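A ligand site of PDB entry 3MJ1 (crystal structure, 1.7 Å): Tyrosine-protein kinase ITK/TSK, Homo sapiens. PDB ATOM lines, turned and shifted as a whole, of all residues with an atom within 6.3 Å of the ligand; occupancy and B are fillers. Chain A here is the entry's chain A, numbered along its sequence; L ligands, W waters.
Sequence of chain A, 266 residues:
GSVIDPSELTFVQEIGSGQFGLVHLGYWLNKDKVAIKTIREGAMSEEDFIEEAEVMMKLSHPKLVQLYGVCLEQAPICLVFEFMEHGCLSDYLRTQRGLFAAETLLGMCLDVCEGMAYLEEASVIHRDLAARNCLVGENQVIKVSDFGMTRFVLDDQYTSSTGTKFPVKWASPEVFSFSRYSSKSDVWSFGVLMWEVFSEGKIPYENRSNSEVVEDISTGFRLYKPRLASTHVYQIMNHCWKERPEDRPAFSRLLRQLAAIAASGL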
ATOM      1  N   ILE A  15      21.863 -13.919  14.772  1.00  0.00           N
ATOM      2  CA  ILE A  15      20.564 -13.868  15.452  1.00  0.00           C
ATOM      3  C   ILE A  15      20.518 -12.854  16.586  1.00  0.00           C
ATOM      4  O   ILE A  15      19.488 -12.675  17.230  1.00  0.00           O
ATOM      5  CB  ILE A  15      20.086 -15.277  15.926  1.00  0.00           C
ATOM      6  CG1 ILE A  15      21.135 -15.924  16.850  1.00  0.00           C
ATOM      7  CG2 ILE A  15      19.743 -16.162  14.731  1.00  0.00           C
ATOM      8  CD1 ILE A  15      20.655 -17.183  17.564  1.00  0.00           C
ATOM      9  N   GLY A  16      21.653 -12.191  16.829  1.00  0.00           N
ATOM     10  CA  GLY A  16      21.736 -11.146  17.838  1.00  0.00           C
ATOM     11  C   GLY A  16      23.125 -10.954  18.424  1.00  0.00           C
ATOM     12  O   GLY A  16      24.078 -11.630  18.041  1.00  0.00           O
ATOM     13  N   SER A  17      23.231  -9.998  19.341  1.00  0.00           N
ATOM     14  CA  SER A  17      24.475  -9.691  20.042  1.00  0.00           C
ATOM     15  C   SER A  17      24.285  -9.780  21.554  1.00  0.00           C
ATOM     16  O   SER A  17      23.221  -9.444  22.077  1.00  0.00           O
ATOM     17  CB  SER A  17      24.973  -8.303  19.658  1.00  0.00           C
ATOM     18  OG  SER A  17      25.326  -8.243  18.295  1.00  0.00           O
ATOM     19  N   GLY A  18      25.327 -10.239  22.236  1.00  0.00           N
ATOM     20  CA  GLY A  18      25.314 -10.346  23.699  1.00  0.00           C
ATOM     21  C   GLY A  18      26.064  -9.203  24.358  1.00  0.00           C
ATOM     22  O   GLY A  18      26.857  -8.517  23.716  1.00  0.00           O
ATOM     23  N   GLY A  21      30.582 -11.534  21.769  1.00  0.00           N
ATOM     24  CA  GLY A  21      29.492 -10.626  21.416  1.00  0.00           C
ATOM     25  C   GLY A  21      28.475 -11.223  20.453  1.00  0.00           C
ATOM     26  O   GLY A  21      27.305 -11.412  20.811  1.00  0.00           O
ATOM     27  N   VAL A  23      26.233 -13.583  18.037  1.00  0.00           N
ATOM     28  CA  VAL A  23      25.593 -14.888  18.169  1.00  0.00           C
ATOM     29  C   VAL A  23      24.963 -15.299  16.838  1.00  0.00           C
ATOM     30  O   VAL A  23      24.202 -14.528  16.242  1.00  0.00           O
ATOM     31  CB  VAL A  23      24.518 -14.910  19.288  1.00  0.00           C
ATOM     32  CG1 VAL A  23      23.890 -16.309  19.431  1.00  0.00           C
ATOM     33  CG2 VAL A  23      25.122 -14.483  20.624  1.00  0.00           C
ATOM     34  N   VAL A  34      22.113 -25.176  16.392  1.00  0.00           N
ATOM     35  CA  VAL A  34      22.886 -24.737  17.559  1.00  0.00           C
ATOM     36  C   VAL A  34      23.051 -23.230  17.527  1.00  0.00           C
ATOM     37  O   VAL A  34      22.970 -22.602  16.461  1.00  0.00           O
ATOM     38  CB  VAL A  34      24.300 -25.394  17.600  1.00  0.00           C
ATOM     39  CG1 VAL A  34      24.219 -26.868  17.947  1.00  0.00           C
ATOM     40  CG2 VAL A  34      25.055 -25.179  16.284  1.00  0.00           C
ATOM     41  N   ALA A  35      23.281 -22.650  18.697  1.00  0.00           N
ATOM     42  CA  ALA A  35      23.642 -21.240  18.800  1.00  0.00           C
ATOM     43  C   ALA A  35      25.140 -21.143  18.990  1.00  0.00           C
ATOM     44  O   ALA A  35      25.701 -21.741  19.921  1.00  0.00           O
ATOM     45  CB  ALA A  35      22.905 -20.585  19.947  1.00  0.00           C
ATOM     46  N   LYS A  37      28.275 -18.841  19.766  1.00  0.00           N
ATOM     47  CA  LYS A  37      28.614 -17.604  20.440  1.00  0.00           C
ATOM     48  C   LYS A  37      30.094 -17.310  20.247  1.00  0.00           C
ATOM     49  O   LYS A  37      30.938 -17.955  20.865  1.00  0.00           O
ATOM     50  CB  LYS A  37      28.264 -17.723  21.924  1.00  0.00           C
ATOM     51  CG  LYS A  37      27.681 -16.472  22.529  1.00  0.00           C
ATOM     52  CD  LYS A  37      26.820 -16.821  23.748  1.00  0.00           C
ATOM     53  CE  LYS A  37      25.899 -15.671  24.122  1.00  0.00           C
ATOM     54  NZ  LYS A  37      24.768 -16.129  24.974  1.00  0.00           N
ATOM     55  N   VAL A  65      20.586 -23.666  29.749  1.00  0.00           N
ATOM     56  CA  VAL A  65      21.012 -23.724  28.357  1.00  0.00           C
ATOM     57  C   VAL A  65      22.356 -24.450  28.302  1.00  0.00           C
ATOM     58  O   VAL A  65      23.327 -24.028  28.913  1.00  0.00           O
ATOM     59  CB  VAL A  65      21.118 -22.325  27.723  1.00  0.00           C
ATOM     60  CG1 VAL A  65      21.520 -22.420  26.249  1.00  0.00           C
ATOM     61  CG2 VAL A  65      19.791 -21.579  27.846  1.00  0.00           C
ATOM     62  N   PHE A  81      26.213 -23.730  21.778  1.00  0.00           N
ATOM     63  CA  PHE A  81      25.131 -23.888  22.746  1.00  0.00           C
ATOM     64  C   PHE A  81      23.888 -24.559  22.178  1.00  0.00           C
ATOM     65  O   PHE A  81      23.659 -24.569  20.962  1.00  0.00           O
ATOM     66  CB  PHE A  81      24.715 -22.530  23.299  1.00  0.00           C
ATOM     67  CG  PHE A  81      25.717 -21.901  24.222  1.00  0.00           C
ATOM     68  CD1 PHE A  81      26.644 -20.993  23.729  1.00  0.00           C
ATOM     69  CD2 PHE A  81      25.709 -22.196  25.574  1.00  0.00           C
ATOM     70  CE1 PHE A  81      27.565 -20.400  24.581  1.00  0.00           C
ATOM     71  CE2 PHE A  81      26.618 -21.611  26.443  1.00  0.00           C
ATOM     72  CZ  PHE A  81      27.550 -20.704  25.942  1.00  0.00           C
ATOM     73  N   GLU A  82      23.083 -25.092  23.090  1.00  0.00           N
ATOM     74  CA  GLU A  82      21.726 -25.527  22.819  1.00  0.00           C
ATOM     75  C   GLU A  82      20.940 -24.384  22.181  1.00  0.00           C
ATOM     76  O   GLU A  82      21.001 -23.239  22.662  1.00  0.00           O
ATOM     77  CB  GLU A  82      21.087 -25.938  24.147  1.00  0.00           C
ATOM     78  CG  GLU A  82      19.621 -26.314  24.085  1.00  0.00           C
ATOM     79  CD  GLU A  82      19.075 -26.692  25.445  1.00  0.00           C
ATOM     80  OE1 GLU A  82      17.938 -27.183  25.499  1.00  0.00           O
ATOM     81  OE2 GLU A  82      19.794 -26.513  26.462  1.00  0.00           O
ATOM     82  N   PHE A  83      20.236 -24.671  21.096  1.00  0.00           N
ATOM     83  CA  PHE A  83      19.450 -23.652  20.405  1.00  0.00           C
ATOM     84  C   PHE A  83      18.062 -23.514  20.988  1.00  0.00           C
ATOM     85  O   PHE A  83      17.306 -24.490  21.073  1.00  0.00           O
ATOM     86  CB  PHE A  83      19.372 -23.896  18.892  1.00  0.00           C
ATOM     87  CG  PHE A  83      18.664 -22.803  18.144  1.00  0.00           C
ATOM     88  CD1 PHE A  83      19.217 -21.530  18.058  1.00  0.00           C
ATOM     89  CD2 PHE A  83      17.430 -23.038  17.535  1.00  0.00           C
ATOM     90  CE1 PHE A  83      18.545 -20.504  17.382  1.00  0.00           C
ATOM     91  CE2 PHE A  83      16.757 -22.022  16.860  1.00  0.00           C
ATOM     92  CZ  PHE A  83      17.318 -20.750  16.779  1.00  0.00           C
ATOM     93  N   MET A  84      17.730 -22.291  21.365  1.00  0.00           N
ATOM     94  CA  MET A  84      16.449 -21.949  21.973  1.00  0.00           C
ATOM     95  C   MET A  84      15.656 -21.101  20.980  1.00  0.00           C
ATOM     96  O   MET A  84      15.942 -19.910  20.778  1.00  0.00           O
ATOM     97  CB  MET A  84      16.661 -21.197  23.285  1.00  0.00           C
ATOM     98  CG  MET A  84      17.566 -21.925  24.272  1.00  0.00           C
ATOM     99  SD  MET A  84      16.865 -23.480  24.852  1.00  0.00           S
ATOM    100  CE  MET A  84      15.555 -22.853  25.914  1.00  0.00           C
ATOM    101  N   GLU A  85      14.640 -21.718  20.384  1.00  0.00           N
ATOM    102  CA  GLU A  85      13.970 -21.166  19.206  1.00  0.00           C
ATOM    103  C   GLU A  85      13.197 -19.868  19.423  1.00  0.00           C
ATOM    104  O   GLU A  85      12.997 -19.110  18.475  1.00  0.00           O
ATOM    105  CB  GLU A  85      13.061 -22.225  18.549  1.00  0.00           C
ATOM    106  CG  GLU A  85      11.860 -22.670  19.365  1.00  0.00           C
ATOM    107  CD  GLU A  85      10.892 -23.517  18.548  1.00  0.00           C
ATOM    108  OE1 GLU A  85      10.747 -23.238  17.340  1.00  0.00           O
ATOM    109  OE2 GLU A  85      10.290 -24.449  19.115  1.00  0.00           O
ATOM    110  N   HIS A  86      12.750 -19.617  20.648  1.00  0.00           N
ATOM    111  CA  HIS A  86      11.908 -18.446  20.913  1.00  0.00           C
ATOM    112  C   HIS A  86      12.650 -17.263  21.524  1.00  0.00           C
ATOM    113  O   HIS A  86      12.030 -16.276  21.918  1.00  0.00           O
ATOM    114  CB  HIS A  86      10.662 -18.820  21.723  1.00  0.00           C
ATOM    115  CG  HIS A  86       9.764 -19.801  21.036  1.00  0.00           C
ATOM    116  ND1 HIS A  86       9.160 -19.539  19.829  1.00  0.00           N
ATOM    117  CD2 HIS A  86       9.372 -21.047  21.395  1.00  0.00           C
ATOM    118  CE1 HIS A  86       8.435 -20.586  19.461  1.00  0.00           C
ATOM    119  NE2 HIS A  86       8.539 -21.509  20.398  1.00  0.00           N
ATOM    120  N   GLY A  87      13.972 -17.358  21.580  1.00  0.00           N
ATOM    121  CA  GLY A  87      14.815 -16.222  21.963  1.00  0.00           C
ATOM    122  C   GLY A  87      14.707 -15.840  23.426  1.00  0.00           C
ATOM    123  O   GLY A  87      14.378 -16.666  24.266  1.00  0.00           O
ATOM    124  N   CYS A  88      14.999 -14.574  23.713  1.00  0.00           N
ATOM    125  CA  CYS A  88      15.089 -14.071  25.083  1.00  0.00           C
ATOM    126  C   CYS A  88      13.727 -14.037  25.761  1.00  0.00           C
ATOM    127  O   CYS A  88      12.716 -13.717  25.122  1.00  0.00           O
ATOM    128  CB  CYS A  88      15.719 -12.668  25.098  1.00  0.00           C
ATOM    129  SG  CYS A  88      17.429 -12.617  24.528  1.00  0.00           S
ATOM    130  N   ASP A  91      12.157 -10.481  25.668  1.00  0.00           N
ATOM    131  CA  ASP A  91      11.522 -10.237  24.359  1.00  0.00           C
ATOM    132  C   ASP A  91      10.213 -10.984  24.220  1.00  0.00           C
ATOM    133  O   ASP A  91       9.228 -10.440  23.708  1.00  0.00           O
ATOM    134  CB  ASP A  91      12.459 -10.647  23.219  1.00  0.00           C
ATOM    135  CG  ASP A  91      13.719  -9.804  23.152  1.00  0.00           C
ATOM    136  OD1 ASP A  91      13.704  -8.634  23.590  1.00  0.00           O
ATOM    137  OD2 ASP A  91      14.737 -10.335  22.643  1.00  0.00           O
ATOM    138  N   ARG A 132      16.278 -11.029  30.442  1.00  0.00           N
ATOM    139  CA  ARG A 132      17.096 -10.886  29.229  1.00  0.00           C
ATOM    140  C   ARG A 132      18.130 -12.012  29.071  1.00  0.00           C
ATOM    141  O   ARG A 132      18.594 -12.283  27.958  1.00  0.00           O
ATOM    142  CB  ARG A 132      17.790  -9.518  29.195  1.00  0.00           C
ATOM    143  CG  ARG A 132      18.793  -9.302  30.309  1.00  0.00           C
ATOM    144  CD  ARG A 132      19.360  -7.887  30.293  1.00  0.00           C
ATOM    145  NE  ARG A 132      19.620  -7.399  31.644  1.00  0.00           N
ATOM    146  CZ  ARG A 132      20.685  -7.728  32.381  1.00  0.00           C
ATOM    147  NH1 ARG A 132      21.603  -8.553  31.903  1.00  0.00           N
ATOM    148  NH2 ARG A 132      20.819  -7.229  33.598  1.00  0.00           N
ATOM    149  N   ASN A 133      18.477 -12.651  30.194  1.00  0.00           N
ATOM    150  CA  ASN A 133      19.457 -13.740  30.213  1.00  0.00           C
ATOM    151  C   ASN A 133      18.833 -15.118  30.392  1.00  0.00           C
ATOM    152  O   ASN A 133      19.529 -16.089  30.711  1.00  0.00           O
ATOM    153  CB  ASN A 133      20.532 -13.479  31.270  1.00  0.00           C
ATOM    154  CG  ASN A 133      21.498 -12.393  30.859  1.00  0.00           C
ATOM    155  OD1 ASN A 133      21.727 -12.169  29.665  1.00  0.00           O
ATOM    156  ND2 ASN A 133      22.075 -11.705  31.842  1.00  0.00           N
ATOM    157  N   LEU A 135      16.243 -17.910  28.240  1.00  0.00           N
ATOM    158  CA  LEU A 135      15.804 -18.218  26.874  1.00  0.00           C
ATOM    159  C   LEU A 135      14.575 -19.121  26.863  1.00  0.00           C
ATOM    160  O   LEU A 135      14.357 -19.886  27.790  1.00  0.00           O
ATOM    161  CB  LEU A 135      16.954 -18.855  26.094  1.00  0.00           C
ATOM    162  CG  LEU A 135      18.143 -17.944  25.775  1.00  0.00           C
ATOM    163  CD1 LEU A 135      19.334 -18.772  25.382  1.00  0.00           C
ATOM    164  CD2 LEU A 135      17.794 -16.956  24.677  1.00  0.00           C
ATOM    165  N   SER A 145      20.474 -18.825  31.053  1.00  0.00           N
ATOM    166  CA  SER A 145      21.611 -18.728  30.131  1.00  0.00           C
ATOM    167  C   SER A 145      22.703 -17.832  30.694  1.00  0.00           C
ATOM    168  O   SER A 145      22.478 -17.093  31.658  1.00  0.00           O
ATOM    169  CB  SER A 145      21.145 -18.204  28.778  1.00  0.00           C
ATOM    170  OG  SER A 145      22.144 -18.356  27.794  1.00  0.00           O
ATOM    171  N   ASP A 146      23.882 -17.888  30.080  1.00  0.00           N
ATOM    172  CA  ASP A 146      24.991 -16.973  30.373  1.00  0.00           C
ATOM    173  C   ASP A 146      25.464 -17.006  31.831  1.00  0.00           C
ATOM    174  O   ASP A 146      25.965 -16.010  32.349  1.00  0.00           O
ATOM    175  CB  ASP A 146      24.659 -15.550  29.917  1.00  0.00           C
ATOM    176  CG  ASP A 146      24.800 -15.358  28.416  1.00  0.00           C
ATOM    177  OD1 ASP A 146      25.289 -16.286  27.731  1.00  0.00           O
ATOM    178  OD2 ASP A 146      24.440 -14.268  27.912  1.00  0.00           O
HETATM  179  N1  LIG L   1      19.101 -16.229  21.051  1.00  0.00           N
HETATM  180  N2  LIG L   1      18.897 -14.853  20.930  1.00  0.00           N
HETATM  181  C1  LIG L   1      18.406 -17.127  20.412  1.00  0.00           C
HETATM  182  C2  LIG L   1      17.924 -14.351  20.141  1.00  0.00           C
HETATM  183  C3  LIG L   1      17.090 -15.286  19.356  1.00  0.00           C
HETATM  184  C4  LIG L   1      17.339 -16.680  19.497  1.00  0.00           C
HETATM  185  C5  LIG L   1      19.645 -19.047  21.382  1.00  0.00           C
HETATM  186  N3  LIG L   1      18.655 -18.491  20.561  1.00  0.00           N
HETATM  187  N4  LIG L   1      19.724 -20.321  21.658  1.00  0.00           N
HETATM  188  C6  LIG L   1      20.714 -18.409  22.034  1.00  0.00           C
HETATM  189  N5  LIG L   1      20.816 -20.540  22.491  1.00  0.00           N
HETATM  190  C7  LIG L   1      21.418 -19.360  22.719  1.00  0.00           C
HETATM  191  N6  LIG L   1      13.178 -14.580  17.517  1.00  0.00           N
HETATM  192  N7  LIG L   1      10.403 -15.060  16.955  1.00  0.00           N
HETATM  193  C8  LIG L   1      16.578 -17.588  18.756  1.00  0.00           C
HETATM  194  C9  LIG L   1      19.748 -13.932  21.705  1.00  0.00           C
HETATM  195  C10 LIG L   1      16.082 -14.840  18.480  1.00  0.00           C
HETATM  196  O1  LIG L   1      17.756 -13.144  20.047  1.00  0.00           O
HETATM  197  C11 LIG L   1      15.344 -15.772  17.770  1.00  0.00           C
HETATM  198  C12 LIG L   1      14.249 -15.321  16.824  1.00  0.00           C
HETATM  199  O2  LIG L   1      22.280 -13.323  22.883  1.00  0.00           O
HETATM  200  C13 LIG L   1      12.349 -15.404  18.424  1.00  0.00           C
HETATM  201  C14 LIG L   1      12.419 -13.675  16.633  1.00  0.00           C
HETATM  202  C15 LIG L   1      11.246 -14.395  15.951  1.00  0.00           C
HETATM  203  C16 LIG L   1      11.167 -16.072  17.714  1.00  0.00           C
HETATM  204  C17 LIG L   1      15.592 -17.126  17.904  1.00  0.00           C
HETATM  205  C18 LIG L   1      20.180 -14.542  23.049  1.00  0.00           C
HETATM  206  C19 LIG L   1      20.992 -13.600  20.851  1.00  0.00           C
HETATM  207  C20 LIG L   1       9.229 -15.686  16.317  1.00  0.00           C
HETATM  208  C21 LIG L   1      21.180 -13.613  23.752  1.00  0.00           C
HETATM  209  C22 LIG L   1      21.934 -12.686  21.652  1.00  0.00           C
HETATM  210  C23 LIG L   1      22.644 -19.157  23.559  1.00  0.00           C
HETATM  211  O   HOH W   1      15.193 -12.709  21.498  1.00  0.00           O
HETATM  212  O   HOH W   2      13.312 -12.361  19.563  1.00  0.00           O
HETATM  213  O   HOH W   3      21.764 -15.779  26.328  1.00  0.00           O
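The backbone carbonyl oxygen (O) of Glu 82 sits at hydrogen-bond distance from a nitrogen (N4) of the ligand, 3.3 Å away. The backbone NH of Met 84 lies close to a nitrogen (N4) of the ligand. O of Met 84 lies within hydrogen-bond range of N3 of the ligand (3.1 Å).
The backbone NH of Phe 81 is in hydrogen-bond range of the backbone carbonyl oxygen of Ala 35 (2.8 Å). The backbone carbonyl oxygen of Val 23 lies within hydrogen-bond range of the backbone NH of Ile 15, 2.8 Å away. The side-chain sulfur (SG) of Cys 88 is in hydrogen-bond range of the backbone carbonyl oxygen (O) of Arg 132, at 3.6 Å. N of Val 23 is in hydrogen-bond range of O of Gly 16 (2.9 Å). The side-chain amino group of Lys 37 is in salt-bridge range of the side-chain carboxylate of Asp 146, at 2.8 Å.
O1 of the ligand lies close to O of Ile 15 (3.3 Å). Merely in contact with the ligand: Gly 16 (3.9 Å), Ser 17 (3.5 Å), Val 23 (3.8 Å), Ala 35 (3.3 Å), Lys 37 (3.96 Å), Phe 81 (3.97 Å), Phe 83 (3.6 Å), Glu 85 (3.3 Å), His 86 (3.6 Å), Gly 87 (3.6 Å), Cys 88 (3.7 Å) and Leu 135 (3.4 Å). Of the 24 residues printed, 15 come within 4 Å of the ligand. The nearest printed residue that does not touch the ligand is Gly 18 (4.2 Å).
Water W1 lies within hydrogen-bond range of the side-chain carboxylate of Asp 91 (2.7 Å), the backbone NH of Cys 88 (2.9 Å) and an oxygen (O1) of the ligand (3.0 Å). Water W3 lies within hydrogen-bond range of OG of Ser 145 (3.0 Å), NZ of Lys 37 (3.3 Å) and OD2 of Asp 146 (3.5 Å).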
